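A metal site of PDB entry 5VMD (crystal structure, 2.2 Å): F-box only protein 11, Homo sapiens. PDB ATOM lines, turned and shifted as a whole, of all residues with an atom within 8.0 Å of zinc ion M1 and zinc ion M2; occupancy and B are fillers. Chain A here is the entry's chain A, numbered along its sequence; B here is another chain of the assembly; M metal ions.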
ATOM      1  N   ALA A  36     -24.430  -5.917 -25.609  1.00  0.00           N
ATOM      2  CA  ALA A  36     -23.174  -5.291 -25.980  1.00  0.00           C
ATOM      3  C   ALA A  36     -22.686  -4.441 -24.817  1.00  0.00           C
ATOM      4  O   ALA A  36     -23.406  -3.563 -24.331  1.00  0.00           O
ATOM      5  CB  ALA A  36     -23.333  -4.437 -27.249  1.00  0.00           C
ATOM      6  N   ILE A  37     -21.449  -4.674 -24.402  1.00  0.00           N
ATOM      7  CA  ILE A  37     -20.878  -4.120 -23.179  1.00  0.00           C
ATOM      8  C   ILE A  37     -19.514  -3.531 -23.492  1.00  0.00           C
ATOM      9  O   ILE A  37     -18.725  -4.146 -24.220  1.00  0.00           O
ATOM     10  CB  ILE A  37     -20.783  -5.211 -22.103  1.00  0.00           C
ATOM     11  CG1 ILE A  37     -22.180  -5.788 -21.816  1.00  0.00           C
ATOM     12  CG2 ILE A  37     -20.087  -4.673 -20.836  1.00  0.00           C
ATOM     13  CD1 ILE A  37     -22.175  -7.072 -21.018  1.00  0.00           C
ATOM     14  N   CYS A  38     -19.225  -2.353 -22.938  1.00  0.00           N
ATOM     15  CA  CYS A  38     -17.948  -1.688 -23.159  1.00  0.00           C
ATOM     16  C   CYS A  38     -16.839  -2.351 -22.346  1.00  0.00           C
ATOM     17  O   CYS A  38     -17.091  -3.126 -21.427  1.00  0.00           O
ATOM     18  CB  CYS A  38     -18.049  -0.197 -22.806  1.00  0.00           C
ATOM     19  SG  CYS A  38     -18.166   0.168 -21.021  1.00  0.00           S
ATOM     20  N   VAL A  39     -15.593  -2.033 -22.714  1.00  0.00           N
ATOM     21  CA  VAL A  39     -14.437  -2.682 -22.092  1.00  0.00           C
ATOM     22  C   VAL A  39     -14.351  -2.323 -20.617  1.00  0.00           C
ATOM     23  O   VAL A  39     -14.011  -3.165 -19.777  1.00  0.00           O
ATOM     24  CB  VAL A  39     -13.135  -2.308 -22.835  1.00  0.00           C
ATOM     25  CG1 VAL A  39     -12.895  -0.813 -22.778  1.00  0.00           C
ATOM     26  CG2 VAL A  39     -11.955  -3.046 -22.213  1.00  0.00           C
ATOM     27  N   ASN A  40     -14.638  -1.063 -20.274  1.00  0.00           N
ATOM     28  CA  ASN A  40     -14.599  -0.652 -18.875  1.00  0.00           C
ATOM     29  C   ASN A  40     -15.621  -1.423 -18.044  1.00  0.00           C
ATOM     30  O   ASN A  40     -15.330  -1.844 -16.921  1.00  0.00           O
ATOM     31  CB  ASN A  40     -14.816   0.860 -18.786  1.00  0.00           C
ATOM     32  CG  ASN A  40     -13.584   1.649 -19.199  1.00  0.00           C
ATOM     33  OD1 ASN A  40     -12.484   1.099 -19.264  1.00  0.00           O
ATOM     34  ND2 ASN A  40     -13.762   2.922 -19.513  1.00  0.00           N
ATOM     35  N   CYS A  41     -16.833  -1.604 -18.572  1.00  0.00           N
ATOM     36  CA  CYS A  41     -17.845  -2.349 -17.835  1.00  0.00           C
ATOM     37  C   CYS A  41     -17.515  -3.825 -17.743  1.00  0.00           C
ATOM     38  O   CYS A  41     -17.742  -4.453 -16.704  1.00  0.00           O
ATOM     39  CB  CYS A  41     -19.234  -2.140 -18.449  1.00  0.00           C
ATOM     40  SG  CYS A  41     -19.969  -0.550 -18.040  1.00  0.00           S
ATOM     41  N   ILE A  42     -16.957  -4.405 -18.809  1.00  0.00           N
ATOM     42  CA  ILE A  42     -16.680  -5.842 -18.747  1.00  0.00           C
ATOM     43  C   ILE A  42     -15.673  -6.121 -17.650  1.00  0.00           C
ATOM     44  O   ILE A  42     -15.750  -7.162 -16.982  1.00  0.00           O
ATOM     45  CB  ILE A  42     -16.216  -6.385 -20.111  1.00  0.00           C
ATOM     46  CG1 ILE A  42     -16.663  -7.842 -20.262  1.00  0.00           C
ATOM     47  CG2 ILE A  42     -14.687  -6.286 -20.252  1.00  0.00           C
ATOM     48  CD1 ILE A  42     -18.205  -7.998 -20.326  1.00  0.00           C
ATOM     49  N   LYS A  43     -14.734  -5.200 -17.430  1.00  0.00           N
ATOM     50  CA  LYS A  43     -13.700  -5.376 -16.408  1.00  0.00           C
ATOM     51  C   LYS A  43     -14.240  -5.134 -15.004  1.00  0.00           C
ATOM     52  O   LYS A  43     -13.995  -5.915 -14.089  1.00  0.00           O
ATOM     53  CB  LYS A  43     -12.518  -4.437 -16.683  1.00  0.00           C
ATOM     54  CG  LYS A  43     -11.715  -4.712 -17.951  1.00  0.00           C
ATOM     55  CD  LYS A  43     -10.434  -3.875 -17.944  1.00  0.00           C
ATOM     56  CE  LYS A  43      -9.371  -4.381 -18.913  1.00  0.00           C
ATOM     57  NZ  LYS A  43      -9.623  -4.025 -20.327  1.00  0.00           N
ATOM     58  N   LYS A  44     -14.981  -4.045 -14.825  1.00  0.00           N
ATOM     59  CA  LYS A  44     -15.423  -3.667 -13.483  1.00  0.00           C
ATOM     60  C   LYS A  44     -16.803  -4.191 -13.136  1.00  0.00           C
ATOM     61  O   LYS A  44     -17.080  -4.452 -11.949  1.00  0.00           O
ATOM     62  CB  LYS A  44     -15.380  -2.152 -13.337  1.00  0.00           C
ATOM     63  CG  LYS A  44     -13.989  -1.574 -13.441  1.00  0.00           C
ATOM     64  CD  LYS A  44     -13.077  -2.238 -12.425  1.00  0.00           C
ATOM     65  CE  LYS A  44     -11.652  -1.711 -12.488  1.00  0.00           C
ATOM     66  NZ  LYS A  44     -10.796  -2.277 -11.395  1.00  0.00           N
ATOM     67  N   CYS A  45     -17.676  -4.386 -14.123  1.00  0.00           N
ATOM     68  CA  CYS A  45     -19.053  -4.791 -13.858  1.00  0.00           C
ATOM     69  C   CYS A  45     -19.320  -6.262 -14.112  1.00  0.00           C
ATOM     70  O   CYS A  45     -20.364  -6.757 -13.680  1.00  0.00           O
ATOM     71  CB  CYS A  45     -20.020  -3.938 -14.692  1.00  0.00           C
ATOM     72  SG  CYS A  45     -19.785  -2.162 -14.485  1.00  0.00           S
ATOM     73  N   HIS A  46     -18.414  -6.982 -14.771  1.00  0.00           N
ATOM     74  CA  HIS A  46     -18.680  -8.386 -15.103  1.00  0.00           C
ATOM     75  C   HIS A  46     -17.466  -9.245 -14.797  1.00  0.00           C
ATOM     76  O   HIS A  46     -17.241 -10.270 -15.454  1.00  0.00           O
ATOM     77  CB  HIS A  46     -19.140  -8.515 -16.561  1.00  0.00           C
ATOM     78  CG  HIS A  46     -20.345  -7.676 -16.872  1.00  0.00           C
ATOM     79  ND1 HIS A  46     -21.636  -8.164 -16.799  1.00  0.00           N
ATOM     80  CD2 HIS A  46     -20.458  -6.366 -17.202  1.00  0.00           C
ATOM     81  CE1 HIS A  46     -22.491  -7.203 -17.095  1.00  0.00           C
ATOM     82  NE2 HIS A  46     -21.796  -6.097 -17.333  1.00  0.00           N
ATOM     83  N   PHE B  59     -20.899   2.942 -29.374  1.00  0.00           N
ATOM     84  CA  PHE B  59     -20.704   3.302 -27.980  1.00  0.00           C
ATOM     85  C   PHE B  59     -21.842   2.834 -27.083  1.00  0.00           C
ATOM     86  O   PHE B  59     -21.796   3.102 -25.868  1.00  0.00           O
ATOM     87  CB  PHE B  59     -20.514   4.822 -27.863  1.00  0.00           C
ATOM     88  CG  PHE B  59     -19.328   5.321 -28.614  1.00  0.00           C
ATOM     89  CD1 PHE B  59     -18.047   4.896 -28.278  1.00  0.00           C
ATOM     90  CD2 PHE B  59     -19.477   6.214 -29.666  1.00  0.00           C
ATOM     91  CE1 PHE B  59     -16.935   5.353 -28.981  1.00  0.00           C
ATOM     92  CE2 PHE B  59     -18.366   6.681 -30.371  1.00  0.00           C
ATOM     93  CZ  PHE B  59     -17.090   6.246 -30.025  1.00  0.00           C
ATOM     94  N   PHE B  60     -22.850   2.145 -27.622  1.00  0.00           N
ATOM     95  CA  PHE B  60     -23.928   1.681 -26.754  1.00  0.00           C
ATOM     96  C   PHE B  60     -23.427   0.574 -25.849  1.00  0.00           C
ATOM     97  O   PHE B  60     -22.701  -0.323 -26.267  1.00  0.00           O
ATOM     98  CB  PHE B  60     -25.114   1.167 -27.564  1.00  0.00           C
ATOM     99  CG  PHE B  60     -26.238   0.654 -26.703  1.00  0.00           C
ATOM    100  CD1 PHE B  60     -27.157   1.537 -26.153  1.00  0.00           C
ATOM    101  CD2 PHE B  60     -26.340  -0.698 -26.392  1.00  0.00           C
ATOM    102  CE1 PHE B  60     -28.199   1.069 -25.334  1.00  0.00           C
ATOM    103  CE2 PHE B  60     -27.375  -1.177 -25.579  1.00  0.00           C
ATOM    104  CZ  PHE B  60     -28.305  -0.289 -25.051  1.00  0.00           C
ATOM    105  N   CYS B  61     -23.848   0.622 -24.592  1.00  0.00           N
ATOM    106  CA  CYS B  61     -23.467  -0.385 -23.610  1.00  0.00           C
ATOM    107  C   CYS B  61     -24.693  -0.791 -22.820  1.00  0.00           C
ATOM    108  O   CYS B  61     -25.271   0.032 -22.111  1.00  0.00           O
ATOM    109  CB  CYS B  61     -22.381   0.129 -22.663  1.00  0.00           C
ATOM    110  SG  CYS B  61     -22.000  -1.045 -21.342  1.00  0.00           S
ATOM    111  N   ASP B  62     -25.075  -2.060 -22.937  1.00  0.00           N
ATOM    112  CA  ASP B  62     -26.209  -2.560 -22.171  1.00  0.00           C
ATOM    113  C   ASP B  62     -25.990  -2.404 -20.669  1.00  0.00           C
ATOM    114  O   ASP B  62     -26.961  -2.172 -19.936  1.00  0.00           O
ATOM    115  CB  ASP B  62     -26.488  -4.022 -22.534  1.00  0.00           C
ATOM    116  CG  ASP B  62     -27.306  -4.145 -23.798  1.00  0.00           C
ATOM    117  OD1 ASP B  62     -28.489  -3.772 -23.745  1.00  0.00           O
ATOM    118  OD2 ASP B  62     -26.782  -4.623 -24.834  1.00  0.00           O
ATOM    119  N   CYS B  63     -24.743  -2.503 -20.194  1.00  0.00           N
ATOM    120  CA  CYS B  63     -24.495  -2.374 -18.757  1.00  0.00           C
ATOM    121  C   CYS B  63     -24.780  -0.951 -18.299  1.00  0.00           C
ATOM    122  O   CYS B  63     -25.626  -0.729 -17.422  1.00  0.00           O
ATOM    123  CB  CYS B  63     -23.051  -2.779 -18.425  1.00  0.00           C
ATOM    124  SG  CYS B  63     -22.705  -2.964 -16.629  1.00  0.00           S
ATOM    125  N   GLY B  64     -24.110   0.026 -18.908  1.00  0.00           N
ATOM    126  CA  GLY B  64     -24.373   1.413 -18.556  1.00  0.00           C
ATOM    127  C   GLY B  64     -25.785   1.848 -18.854  1.00  0.00           C
ATOM    128  O   GLY B  64     -26.313   2.752 -18.190  1.00  0.00           O
ATOM    129  N   ALA B  65     -26.433   1.222 -19.842  1.00  0.00           N
ATOM    130  CA  ALA B  65     -27.824   1.553 -20.166  1.00  0.00           C
ATOM    131  C   ALA B  65     -28.813   1.013 -19.152  1.00  0.00           C
ATOM    132  O   ALA B  65     -29.997   1.378 -19.200  1.00  0.00           O
ATOM    133  CB  ALA B  65     -28.191   1.037 -21.564  1.00  0.00           C
ATOM    134  N   GLY B  66     -28.379   0.144 -18.239  1.00  0.00           N
ATOM    135  CA  GLY B  66     -29.281  -0.395 -17.223  1.00  0.00           C
ATOM    136  C   GLY B  66     -30.178  -1.524 -17.672  1.00  0.00           C
ATOM    137  O   GLY B  66     -31.224  -1.732 -17.062  1.00  0.00           O
ATOM    138  N   LEU B  68     -29.125  -4.788 -17.884  1.00  0.00           N
ATOM    139  CA  LEU B  68     -28.659  -6.055 -17.344  1.00  0.00           C
ATOM    140  C   LEU B  68     -29.203  -6.230 -15.924  1.00  0.00           C
ATOM    141  O   LEU B  68     -29.669  -5.282 -15.292  1.00  0.00           O
ATOM    142  CB  LEU B  68     -27.129  -6.109 -17.361  1.00  0.00           C
ATOM    143  CG  LEU B  68     -26.563  -5.835 -18.758  1.00  0.00           C
ATOM    144  CD1 LEU B  68     -25.037  -5.874 -18.742  1.00  0.00           C
ATOM    145  CD2 LEU B  68     -27.115  -6.823 -19.784  1.00  0.00           C
ATOM    146  N   ASN B  70     -27.817  -6.644 -13.061  1.00  0.00           N
ATOM    147  CA  ASN B  70     -27.228  -5.830 -12.006  1.00  0.00           C
ATOM    148  C   ASN B  70     -26.967  -4.405 -12.491  1.00  0.00           C
ATOM    149  O   ASN B  70     -26.616  -4.201 -13.656  1.00  0.00           O
ATOM    150  CB  ASN B  70     -25.910  -6.439 -11.516  1.00  0.00           C
ATOM    151  CG  ASN B  70     -26.078  -7.854 -10.988  1.00  0.00           C
ATOM    152  OD1 ASN B  70     -27.061  -8.167 -10.323  1.00  0.00           O
ATOM    153  ND2 ASN B  70     -25.122  -8.722 -11.298  1.00  0.00           N
ATOM    154  N   PRO B  71     -27.085  -3.401 -11.628  1.00  0.00           N
ATOM    155  CA  PRO B  71     -26.817  -2.026 -12.054  1.00  0.00           C
ATOM    156  C   PRO B  71     -25.341  -1.821 -12.367  1.00  0.00           C
ATOM    157  O   PRO B  71     -24.465  -2.475 -11.792  1.00  0.00           O
ATOM    158  CB  PRO B  71     -27.236  -1.176 -10.842  1.00  0.00           C
ATOM    159  CG  PRO B  71     -28.096  -2.096  -9.991  1.00  0.00           C
ATOM    160  CD  PRO B  71     -27.543  -3.465 -10.228  1.00  0.00           C
ATOM    161  N   CYS B  72     -25.068  -0.911 -13.293  1.00  0.00           N
ATOM    162  CA  CYS B  72     -23.684  -0.617 -13.669  1.00  0.00           C
ATOM    163  C   CYS B  72     -22.946   0.003 -12.490  1.00  0.00           C
ATOM    164  O   CYS B  72     -23.479   0.872 -11.789  1.00  0.00           O
ATOM    165  CB  CYS B  72     -23.654   0.336 -14.867  1.00  0.00           C
ATOM    166  SG  CYS B  72     -22.000   0.891 -15.361  1.00  0.00           S
ATOM    167  N   THR B  73     -21.698  -0.400 -12.291  1.00  0.00           N
ATOM    168  CA  THR B  73     -20.912   0.133 -11.182  1.00  0.00           C
ATOM    169  C   THR B  73     -20.127   1.378 -11.576  1.00  0.00           C
ATOM    170  O   THR B  73     -19.483   1.981 -10.714  1.00  0.00           O
ATOM    171  CB  THR B  73     -19.936  -0.924 -10.652  1.00  0.00           C
ATOM    172  OG1 THR B  73     -18.828  -1.065 -11.552  1.00  0.00           O
ATOM    173  CG2 THR B  73     -20.637  -2.263 -10.513  1.00  0.00           C
ATOM    174  N   LEU B  74     -20.202   1.784 -12.836  1.00  0.00           N
ATOM    175  CA  LEU B  74     -19.452   2.936 -13.323  1.00  0.00           C
ATOM    176  C   LEU B  74     -20.366   4.158 -13.544  1.00  0.00           C
ATOM    177  O   LEU B  74     -21.547   4.141 -13.200  1.00  0.00           O
ATOM    178  CB  LEU B  74     -18.730   2.573 -14.620  1.00  0.00           C
ATOM    179  CG  LEU B  74     -17.745   1.414 -14.450  1.00  0.00           C
ATOM    180  CD1 LEU B  74     -17.078   1.048 -15.775  1.00  0.00           C
ATOM    181  CD2 LEU B  74     -16.691   1.741 -13.375  1.00  0.00           C
HETATM  182 ZN    ZN M   1     -21.283  -1.201 -16.173  1.00  0.00          ZN
HETATM  183 ZN    ZN M   2     -20.424   0.343 -20.219  1.00  0.00          ZN
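Zinc ion M2 is bound by the side-chain sulfur (SG) of Cys 61 of chain B (2.4 Å), the side-chain sulfur (SG) of Cys 41 (2.4 Å) and the side-chain sulfur (SG) of Cys 38 (2.4 Å).
Zinc ion M1 is bound by the side-chain sulfur of Cys 63 of chain B (2.3 Å), the side-chain sulfur of Cys 72 of chain B (2.4 Å), the side-chain sulfur of Cys 41 (2.4 Å) and the side-chain sulfur of Cys 45 (2.5 Å).
The backbone NH (N) of Cys 63 of chain B lies close to the side-chain sulfur (SG) of Cys 61 of chain B (3.3 Å).
SG of Cys 63 of chain B sits close to NE2 of His 46 (3.3 Å).
The side-chain sulfur of Cys 72 of chain B lies close to the backbone NH of Leu 74 of chain B (3.2 Å).
The backbone carbonyl oxygen (O) of Cys 41 lies within hydrogen-bond range of the backbone NH (N) of His 46 (3.3 Å).
The backbone NH (N) of Gly 64 of chain B sits close to the side-chain sulfur (SG) of Cys 61 of chain B (3.4 Å).
The side-chain sulfur of Cys 45 sits close to the side-chain hydroxyl of Thr 73 of chain B, 3.3 Å away.
Residues that only touch zinc ion M1: Thr 73 of chain B.
N of Gly 64 of chain B touches zinc ion M2, at 3.9 Å.
Four residues have an atom within 4 Å of zinc ion M2: Cys 38, Cys 41, Cys 61 of chain B and Gly 64 of chain B.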
